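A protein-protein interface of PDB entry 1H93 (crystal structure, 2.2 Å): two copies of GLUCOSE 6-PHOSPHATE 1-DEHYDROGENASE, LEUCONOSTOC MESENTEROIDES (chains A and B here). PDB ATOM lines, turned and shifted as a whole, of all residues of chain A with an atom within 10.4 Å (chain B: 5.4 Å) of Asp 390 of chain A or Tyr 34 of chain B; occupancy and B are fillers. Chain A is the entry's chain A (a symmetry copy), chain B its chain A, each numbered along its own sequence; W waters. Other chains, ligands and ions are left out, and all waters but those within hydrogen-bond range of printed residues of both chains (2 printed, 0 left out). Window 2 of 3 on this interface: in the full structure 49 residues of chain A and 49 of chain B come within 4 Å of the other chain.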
ATOM      1  N   SER A 360     -17.784   4.951   0.463  1.00  0.00           N
ATOM      2  CA  SER A 360     -17.566   4.560   1.853  1.00  0.00           C
ATOM      3  C   SER A 360     -18.463   5.313   2.825  1.00  0.00           C
ATOM      4  O   SER A 360     -19.127   6.281   2.443  1.00  0.00           O
ATOM      5  CB  SER A 360     -16.098   4.790   2.221  1.00  0.00           C
ATOM      6  OG  SER A 360     -15.602   5.974   1.618  1.00  0.00           O
ATOM      7  N   LYS A 386      -6.507   5.323   3.755  1.00  0.00           N
ATOM      8  CA  LYS A 386      -7.441   4.227   3.984  1.00  0.00           C
ATOM      9  C   LYS A 386      -7.379   3.794   5.436  1.00  0.00           C
ATOM     10  O   LYS A 386      -6.289   3.643   5.999  1.00  0.00           O
ATOM     11  CB  LYS A 386      -7.098   3.031   3.087  1.00  0.00           C
ATOM     12  CG  LYS A 386      -8.089   1.875   3.181  1.00  0.00           C
ATOM     13  CD  LYS A 386      -7.524   0.595   2.566  1.00  0.00           C
ATOM     14  CE  LYS A 386      -8.544  -0.545   2.626  1.00  0.00           C
ATOM     15  NZ  LYS A 386      -8.919  -0.897   4.019  1.00  0.00           N
ATOM     16  N   SER A 387      -8.542   3.612   6.050  1.00  0.00           N
ATOM     17  CA  SER A 387      -8.597   3.164   7.434  1.00  0.00           C
ATOM     18  C   SER A 387      -8.306   1.663   7.480  1.00  0.00           C
ATOM     19  O   SER A 387      -8.466   0.970   6.475  1.00  0.00           O
ATOM     20  CB  SER A 387      -9.980   3.431   8.015  1.00  0.00           C
ATOM     21  OG  SER A 387     -10.981   2.780   7.252  1.00  0.00           O
ATOM     22  N   VAL A 388      -7.834   1.166   8.619  1.00  0.00           N
ATOM     23  CA  VAL A 388      -7.564  -0.260   8.745  1.00  0.00           C
ATOM     24  C   VAL A 388      -8.864  -0.927   9.195  1.00  0.00           C
ATOM     25  O   VAL A 388      -9.090  -1.173  10.385  1.00  0.00           O
ATOM     26  CB  VAL A 388      -6.418  -0.545   9.741  1.00  0.00           C
ATOM     27  CG1 VAL A 388      -6.307  -2.036  10.007  1.00  0.00           C
ATOM     28  CG2 VAL A 388      -5.099  -0.031   9.171  1.00  0.00           C
ATOM     29  N   GLU A 389      -9.760  -1.108   8.233  1.00  0.00           N
ATOM     30  CA  GLU A 389     -11.053  -1.725   8.467  1.00  0.00           C
ATOM     31  C   GLU A 389     -11.253  -2.765   7.376  1.00  0.00           C
ATOM     32  O   GLU A 389     -10.492  -2.803   6.408  1.00  0.00           O
ATOM     33  CB  GLU A 389     -12.158  -0.674   8.423  1.00  0.00           C
ATOM     34  CG  GLU A 389     -12.111   0.298   9.589  1.00  0.00           C
ATOM     35  CD  GLU A 389     -13.275   1.266   9.584  1.00  0.00           C
ATOM     36  OE1 GLU A 389     -13.363   2.078   8.641  1.00  0.00           O
ATOM     37  OE2 GLU A 389     -14.106   1.212  10.518  1.00  0.00           O
ATOM     38  N   ASP A 390     -12.255  -3.624   7.532  1.00  0.00           N
ATOM     39  CA  ASP A 390     -12.490  -4.672   6.540  1.00  0.00           C
ATOM     40  C   ASP A 390     -13.060  -4.135   5.235  1.00  0.00           C
ATOM     41  O   ASP A 390     -12.597  -4.500   4.156  1.00  0.00           O
ATOM     42  CB  ASP A 390     -13.344  -5.802   7.127  1.00  0.00           C
ATOM     43  CG  ASP A 390     -12.584  -6.627   8.167  1.00  0.00           C
ATOM     44  OD1 ASP A 390     -11.339  -6.742   8.062  1.00  0.00           O
ATOM     45  OD2 ASP A 390     -13.222  -7.153   9.097  1.00  0.00           O
ATOM     46  N   ALA A 391     -14.033  -3.238   5.342  1.00  0.00           N
ATOM     47  CA  ALA A 391     -14.655  -2.621   4.180  1.00  0.00           C
ATOM     48  C   ALA A 391     -13.853  -1.361   3.867  1.00  0.00           C
ATOM     49  O   ALA A 391     -13.303  -0.728   4.773  1.00  0.00           O
ATOM     50  CB  ALA A 391     -16.105  -2.261   4.482  1.00  0.00           C
ATOM     51  N   PHE A 392     -13.780  -0.998   2.591  1.00  0.00           N
ATOM     52  CA  PHE A 392     -13.031   0.186   2.206  1.00  0.00           C
ATOM     53  C   PHE A 392     -13.628   1.439   2.848  1.00  0.00           C
ATOM     54  O   PHE A 392     -14.836   1.688   2.742  1.00  0.00           O
ATOM     55  CB  PHE A 392     -12.988   0.351   0.684  1.00  0.00           C
ATOM     56  CG  PHE A 392     -12.107   1.484   0.237  1.00  0.00           C
ATOM     57  CD1 PHE A 392     -10.748   1.281   0.031  1.00  0.00           C
ATOM     58  CD2 PHE A 392     -12.623   2.768   0.091  1.00  0.00           C
ATOM     59  CE1 PHE A 392      -9.917   2.337  -0.310  1.00  0.00           C
ATOM     60  CE2 PHE A 392     -11.795   3.831  -0.247  1.00  0.00           C
ATOM     61  CZ  PHE A 392     -10.442   3.614  -0.447  1.00  0.00           C
ATOM     62  N   ASN A 393     -12.774   2.239   3.481  1.00  0.00           N
ATOM     63  CA  ASN A 393     -13.214   3.459   4.142  1.00  0.00           C
ATOM     64  C   ASN A 393     -12.032   4.401   4.296  1.00  0.00           C
ATOM     65  O   ASN A 393     -10.885   3.948   4.395  1.00  0.00           O
ATOM     66  CB  ASN A 393     -13.787   3.125   5.514  1.00  0.00           C
ATOM     67  CG  ASN A 393     -14.686   4.203   6.038  1.00  0.00           C
ATOM     68  OD1 ASN A 393     -15.395   4.852   5.276  1.00  0.00           O
ATOM     69  ND2 ASN A 393     -14.685   4.393   7.349  1.00  0.00           N
ATOM     70  N   THR A 394     -12.300   5.706   4.308  1.00  0.00           N
ATOM     71  CA  THR A 394     -11.233   6.688   4.443  1.00  0.00           C
ATOM     72  C   THR A 394     -11.111   7.220   5.870  1.00  0.00           C
ATOM     73  O   THR A 394     -12.019   7.075   6.694  1.00  0.00           O
ATOM     74  CB  THR A 394     -11.421   7.877   3.460  1.00  0.00           C
ATOM     75  OG1 THR A 394     -12.564   8.650   3.839  1.00  0.00           O
ATOM     76  CG2 THR A 394     -11.628   7.367   2.037  1.00  0.00           C
ATOM     77  N   VAL B   1     -22.245  -8.453  12.506  1.00  0.00           N
ATOM     78  CA  VAL B   1     -22.122  -7.997  11.089  1.00  0.00           C
ATOM     79  C   VAL B   1     -23.018  -8.863  10.207  1.00  0.00           C
ATOM     80  O   VAL B   1     -23.617  -9.825  10.696  1.00  0.00           O
ATOM     81  CB  VAL B   1     -20.658  -8.096  10.590  1.00  0.00           C
ATOM     82  CG1 VAL B   1     -19.772  -7.132  11.361  1.00  0.00           C
ATOM     83  CG2 VAL B   1     -20.142  -9.516  10.744  1.00  0.00           C
ATOM     84  N   SER B   2     -23.132  -8.507   8.929  1.00  0.00           N
ATOM     85  CA  SER B   2     -23.945  -9.272   7.984  1.00  0.00           C
ATOM     86  C   SER B   2     -23.312 -10.638   7.712  1.00  0.00           C
ATOM     87  O   SER B   2     -22.125 -10.730   7.376  1.00  0.00           O
ATOM     88  CB  SER B   2     -24.112  -8.503   6.669  1.00  0.00           C
ATOM     89  OG  SER B   2     -24.772  -7.268   6.889  1.00  0.00           O
ATOM     90  N   GLU B   3     -24.109 -11.691   7.869  1.00  0.00           N
ATOM     91  CA  GLU B   3     -23.651 -13.065   7.655  1.00  0.00           C
ATOM     92  C   GLU B   3     -23.271 -13.345   6.205  1.00  0.00           C
ATOM     93  O   GLU B   3     -24.008 -12.991   5.284  1.00  0.00           O
ATOM     94  CB  GLU B   3     -24.741 -14.051   8.099  1.00  0.00           C
ATOM     95  CG  GLU B   3     -24.381 -15.528   7.944  1.00  0.00           C
ATOM     96  CD  GLU B   3     -25.485 -16.475   8.412  1.00  0.00           C
ATOM     97  OE1 GLU B   3     -26.670 -16.069   8.454  1.00  0.00           O
ATOM     98  OE2 GLU B   3     -25.162 -17.635   8.734  1.00  0.00           O
ATOM     99  N   ILE B   4     -22.101 -13.946   6.010  1.00  0.00           N
ATOM    100  CA  ILE B   4     -21.632 -14.314   4.676  1.00  0.00           C
ATOM    101  C   ILE B   4     -22.006 -15.781   4.460  1.00  0.00           C
ATOM    102  O   ILE B   4     -21.460 -16.674   5.112  1.00  0.00           O
ATOM    103  CB  ILE B   4     -20.093 -14.149   4.520  1.00  0.00           C
ATOM    104  CG1 ILE B   4     -19.703 -12.666   4.579  1.00  0.00           C
ATOM    105  CG2 ILE B   4     -19.623 -14.776   3.204  1.00  0.00           C
ATOM    106  CD1 ILE B   4     -18.221 -12.401   4.350  1.00  0.00           C
ATOM    107  N   ASN B  28     -10.374 -16.613  10.621  1.00  0.00           N
ATOM    108  CA  ASN B  28     -10.524 -15.215  11.007  1.00  0.00           C
ATOM    109  C   ASN B  28     -11.874 -14.670  10.604  1.00  0.00           C
ATOM    110  O   ASN B  28     -12.511 -13.969  11.383  1.00  0.00           O
ATOM    111  CB  ASN B  28      -9.424 -14.352  10.401  1.00  0.00           C
ATOM    112  CG  ASN B  28      -8.246 -14.178  11.332  1.00  0.00           C
ATOM    113  OD1 ASN B  28      -8.390 -13.707  12.465  1.00  0.00           O
ATOM    114  ND2 ASN B  28      -7.064 -14.536  10.852  1.00  0.00           N
ATOM    115  N   LEU B  29     -12.329 -15.011   9.400  1.00  0.00           N
ATOM    116  CA  LEU B  29     -13.632 -14.543   8.937  1.00  0.00           C
ATOM    117  C   LEU B  29     -14.745 -15.062   9.842  1.00  0.00           C
ATOM    118  O   LEU B  29     -15.795 -14.431   9.971  1.00  0.00           O
ATOM    119  CB  LEU B  29     -13.877 -14.956   7.487  1.00  0.00           C
ATOM    120  CG  LEU B  29     -12.922 -14.289   6.494  1.00  0.00           C
ATOM    121  CD1 LEU B  29     -13.219 -14.747   5.082  1.00  0.00           C
ATOM    122  CD2 LEU B  29     -13.056 -12.776   6.603  1.00  0.00           C
ATOM    123  N   TYR B  30     -14.502 -16.208  10.473  1.00  0.00           N
ATOM    124  CA  TYR B  30     -15.461 -16.811  11.392  1.00  0.00           C
ATOM    125  C   TYR B  30     -15.365 -16.078  12.738  1.00  0.00           C
ATOM    126  O   TYR B  30     -16.380 -15.685  13.320  1.00  0.00           O
ATOM    127  CB  TYR B  30     -15.154 -18.307  11.573  1.00  0.00           C
ATOM    128  CG  TYR B  30     -16.133 -19.043  12.467  1.00  0.00           C
ATOM    129  CD1 TYR B  30     -17.438 -19.287  12.047  1.00  0.00           C
ATOM    130  CD2 TYR B  30     -15.754 -19.494  13.732  1.00  0.00           C
ATOM    131  CE1 TYR B  30     -18.352 -19.964  12.863  1.00  0.00           C
ATOM    132  CE2 TYR B  30     -16.659 -20.176  14.562  1.00  0.00           C
ATOM    133  CZ  TYR B  30     -17.957 -20.407  14.119  1.00  0.00           C
ATOM    134  OH  TYR B  30     -18.855 -21.082  14.923  1.00  0.00           O
ATOM    135  N   LYS B  32     -14.413 -13.161  13.271  1.00  0.00           N
ATOM    136  CA  LYS B  32     -14.910 -11.802  13.093  1.00  0.00           C
ATOM    137  C   LYS B  32     -16.429 -11.775  12.920  1.00  0.00           C
ATOM    138  O   LYS B  32     -17.008 -10.716  12.671  1.00  0.00           O
ATOM    139  CB  LYS B  32     -14.234 -11.130  11.894  1.00  0.00           C
ATOM    140  CG  LYS B  32     -12.771 -10.752  12.120  1.00  0.00           C
ATOM    141  CD  LYS B  32     -12.156 -10.057  10.899  1.00  0.00           C
ATOM    142  CE  LYS B  32     -10.836  -9.372  11.264  1.00  0.00           C
ATOM    143  NZ  LYS B  32     -10.155  -8.714  10.117  1.00  0.00           N
ATOM    144  N   GLY B  33     -17.066 -12.942  13.017  1.00  0.00           N
ATOM    145  CA  GLY B  33     -18.513 -13.022  12.886  1.00  0.00           C
ATOM    146  C   GLY B  33     -19.119 -12.981  11.488  1.00  0.00           C
ATOM    147  O   GLY B  33     -20.341 -12.917  11.356  1.00  0.00           O
ATOM    148  N   TYR B  34     -18.293 -12.991  10.445  1.00  0.00           N
ATOM    149  CA  TYR B  34     -18.801 -12.965   9.069  1.00  0.00           C
ATOM    150  C   TYR B  34     -19.417 -14.317   8.752  1.00  0.00           C
ATOM    151  O   TYR B  34     -20.576 -14.411   8.348  1.00  0.00           O
ATOM    152  CB  TYR B  34     -17.670 -12.666   8.083  1.00  0.00           C
ATOM    153  CG  TYR B  34     -17.121 -11.270   8.215  1.00  0.00           C
ATOM    154  CD1 TYR B  34     -17.866 -10.173   7.782  1.00  0.00           C
ATOM    155  CD2 TYR B  34     -15.873 -11.037   8.790  1.00  0.00           C
ATOM    156  CE1 TYR B  34     -17.391  -8.885   7.917  1.00  0.00           C
ATOM    157  CE2 TYR B  34     -15.384  -9.741   8.929  1.00  0.00           C
ATOM    158  CZ  TYR B  34     -16.153  -8.675   8.490  1.00  0.00           C
ATOM    159  OH  TYR B  34     -15.704  -7.388   8.618  1.00  0.00           O
ATOM    160  N   LEU B  35     -18.611 -15.358   8.918  1.00  0.00           N
ATOM    161  CA  LEU B  35     -19.044 -16.727   8.699  1.00  0.00           C
ATOM    162  C   LEU B  35     -19.695 -17.155  10.012  1.00  0.00           C
ATOM    163  O   LEU B  35     -19.076 -17.062  11.073  1.00  0.00           O
ATOM    164  CB  LEU B  35     -17.833 -17.607   8.383  1.00  0.00           C
ATOM    165  CG  LEU B  35     -17.470 -17.843   6.911  1.00  0.00           C
ATOM    166  CD1 LEU B  35     -17.755 -16.633   6.057  1.00  0.00           C
ATOM    167  CD2 LEU B  35     -16.013 -18.256   6.811  1.00  0.00           C
ATOM    168  N   GLN B  36     -20.964 -17.538   9.950  1.00  0.00           N
ATOM    169  CA  GLN B  36     -21.700 -17.949  11.145  1.00  0.00           C
ATOM    170  C   GLN B  36     -22.255 -19.374  11.042  1.00  0.00           C
ATOM    171  O   GLN B  36     -21.597 -20.330  11.450  1.00  0.00           O
ATOM    172  CB  GLN B  36     -22.828 -16.952  11.422  1.00  0.00           C
ATOM    173  CG  GLN B  36     -22.364 -15.512  11.550  1.00  0.00           C
ATOM    174  CD  GLN B  36     -23.503 -14.519  11.457  1.00  0.00           C
ATOM    175  OE1 GLN B  36     -24.663 -14.860  11.691  1.00  0.00           O
ATOM    176  NE2 GLN B  36     -23.183 -13.287  11.091  1.00  0.00           N
ATOM    177  N   PRO B 412      -5.751  -6.914   8.174  1.00  0.00           N
ATOM    178  CA  PRO B 412      -5.997  -8.259   7.651  1.00  0.00           C
ATOM    179  C   PRO B 412      -4.856  -8.697   6.728  1.00  0.00           C
ATOM    180  O   PRO B 412      -4.304  -7.884   5.972  1.00  0.00           O
ATOM    181  CB  PRO B 412      -7.295  -8.081   6.856  1.00  0.00           C
ATOM    182  CG  PRO B 412      -7.961  -6.916   7.527  1.00  0.00           C
ATOM    183  CD  PRO B 412      -6.802  -5.985   7.728  1.00  0.00           C
ATOM    184  N   GLU B 416      -6.670 -13.360   3.641  1.00  0.00           N
ATOM    185  CA  GLU B 416      -7.969 -13.165   4.281  1.00  0.00           C
ATOM    186  C   GLU B 416      -8.739 -12.130   3.470  1.00  0.00           C
ATOM    187  O   GLU B 416      -9.955 -12.243   3.271  1.00  0.00           O
ATOM    188  CB  GLU B 416      -7.807 -12.666   5.722  1.00  0.00           C
ATOM    189  CG  GLU B 416      -9.136 -12.510   6.464  1.00  0.00           C
ATOM    190  CD  GLU B 416      -9.023 -11.748   7.785  1.00  0.00           C
ATOM    191  OE1 GLU B 416      -7.997 -11.879   8.483  1.00  0.00           O
ATOM    192  OE2 GLU B 416      -9.981 -11.027   8.131  1.00  0.00           O
ATOM    193  N   ARG B 417      -8.011 -11.118   3.003  1.00  0.00           N
ATOM    194  CA  ARG B 417      -8.588 -10.044   2.205  1.00  0.00           C
ATOM    195  C   ARG B 417      -9.109 -10.621   0.892  1.00  0.00           C
ATOM    196  O   ARG B 417     -10.275 -10.443   0.556  1.00  0.00           O
ATOM    197  CB  ARG B 417      -7.528  -8.962   1.933  1.00  0.00           C
ATOM    198  CG  ARG B 417      -8.056  -7.637   1.371  1.00  0.00           C
ATOM    199  CD  ARG B 417      -8.922  -6.875   2.383  1.00  0.00           C
ATOM    200  NE  ARG B 417     -10.354  -7.023   2.117  1.00  0.00           N
ATOM    201  CZ  ARG B 417     -11.235  -7.563   2.958  1.00  0.00           C
ATOM    202  NH1 ARG B 417     -10.848  -8.013   4.144  1.00  0.00           N
ATOM    203  NH2 ARG B 417     -12.506  -7.675   2.599  1.00  0.00           N
ATOM    204  N   HIS B 420     -12.055 -12.989   1.410  1.00  0.00           N
ATOM    205  CA  HIS B 420     -13.175 -12.162   1.846  1.00  0.00           C
ATOM    206  C   HIS B 420     -13.772 -11.377   0.683  1.00  0.00           C
ATOM    207  O   HIS B 420     -14.996 -11.266   0.566  1.00  0.00           O
ATOM    208  CB  HIS B 420     -12.712 -11.193   2.934  1.00  0.00           C
ATOM    209  CG  HIS B 420     -13.833 -10.556   3.693  1.00  0.00           C
ATOM    210  ND1 HIS B 420     -13.641  -9.905   4.893  1.00  0.00           N
ATOM    211  CD2 HIS B 420     -15.163 -10.498   3.445  1.00  0.00           C
ATOM    212  CE1 HIS B 420     -14.805  -9.480   5.353  1.00  0.00           C
ATOM    213  NE2 HIS B 420     -15.742  -9.830   4.493  1.00  0.00           N
HETATM  214  O   HOH W   1     -14.972  -6.301   3.528  1.00  0.00           O
HETATM  215  O   HOH W   2     -11.395  -9.418   6.294  1.00  0.00           O
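The side-chain carboxylate (OE2) of Glu 416 of chain B lies within salt-bridge range of the side-chain amino group (NZ) of Lys 32 of chain B.
NH2 of Arg 417 of chain B sits close to ND1 of His 420 of chain B (3.4 Å).
The backbone NH (N) of Ile 4 of chain B is in hydrogen-bond range of the backbone carbonyl oxygen (O) of Tyr 34 of chain B (2.8 Å).
N of Tyr 34 of chain B sits at hydrogen-bond distance from O of Leu 29 of chain B, 2.9 Å away.
The side-chain hydroxyl (OH) of Tyr 34 of chain B sits at hydrogen-bond distance from the side-chain carboxylate (OD2) of Asp 390 of chain A (2.5 Å).
The side-chain carboxylate (OD1) of Asp 390 of chain A is in salt-bridge range of the side-chain amino group (NZ) of Lys 32 of chain B (3.1 Å).
Among the printed residues, merely in contact across the chains: Asp 390 of chain A with Pro 412 of chain B (3.4 Å) and Asp 390 of chain A with Arg 417 of chain B (3.5 Å).
Of the 10 printed residues of chain A, 1 touches a printed residue of chain B.
Printed residues of chain A that touch a printed residue of chain B: Asp 390.
No position is printed for both chains.
Asp 390 of chain A touches just these residues of chain B: Lys 32, Tyr 34, Pro 412 and Arg 417.
Tyr 34 of chain B touches one residue of chain A.
No residue of chain A comes within 4 Å of Ile 4 of chain B.
No residue of chain A comes within 4 Å of Leu 29 of chain B.
Of chain A, only Asp 390 (3.1 Å) comes within 4 Å of Lys 32 of chain B.
No residue of chain A comes within 4 Å of Gly 33 of chain B.
No residue of chain A comes within 4 Å of Leu 35 of chain B.
Of the printed residues of chain A, Arg 417 of chain B touches Asp 390.
Of the printed residues of chain A, Pro 412 of chain B touches Asp 390 (3.4 Å).
The nearest printed residue of chain A that does not touch Arg 417 of chain B is Ala 391 of chain A (5.4 Å).
Water W2 lies within hydrogen-bond range of the guanidinium group (NH1) of Arg 417 of chain B, a ring nitrogen (ND1) of His 420 of chain B, the side-chain carboxylate (OE2) of Glu 416 of chain B and the side-chain carboxylate (OD1) of Asp 390 of chain A.
Water W1 bridges the guanidinium group (NH2) of Arg 417 of chain B (3.0 Å) and the backbone carbonyl oxygen (O) of Asp 390 of chain A (3.0 Å).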
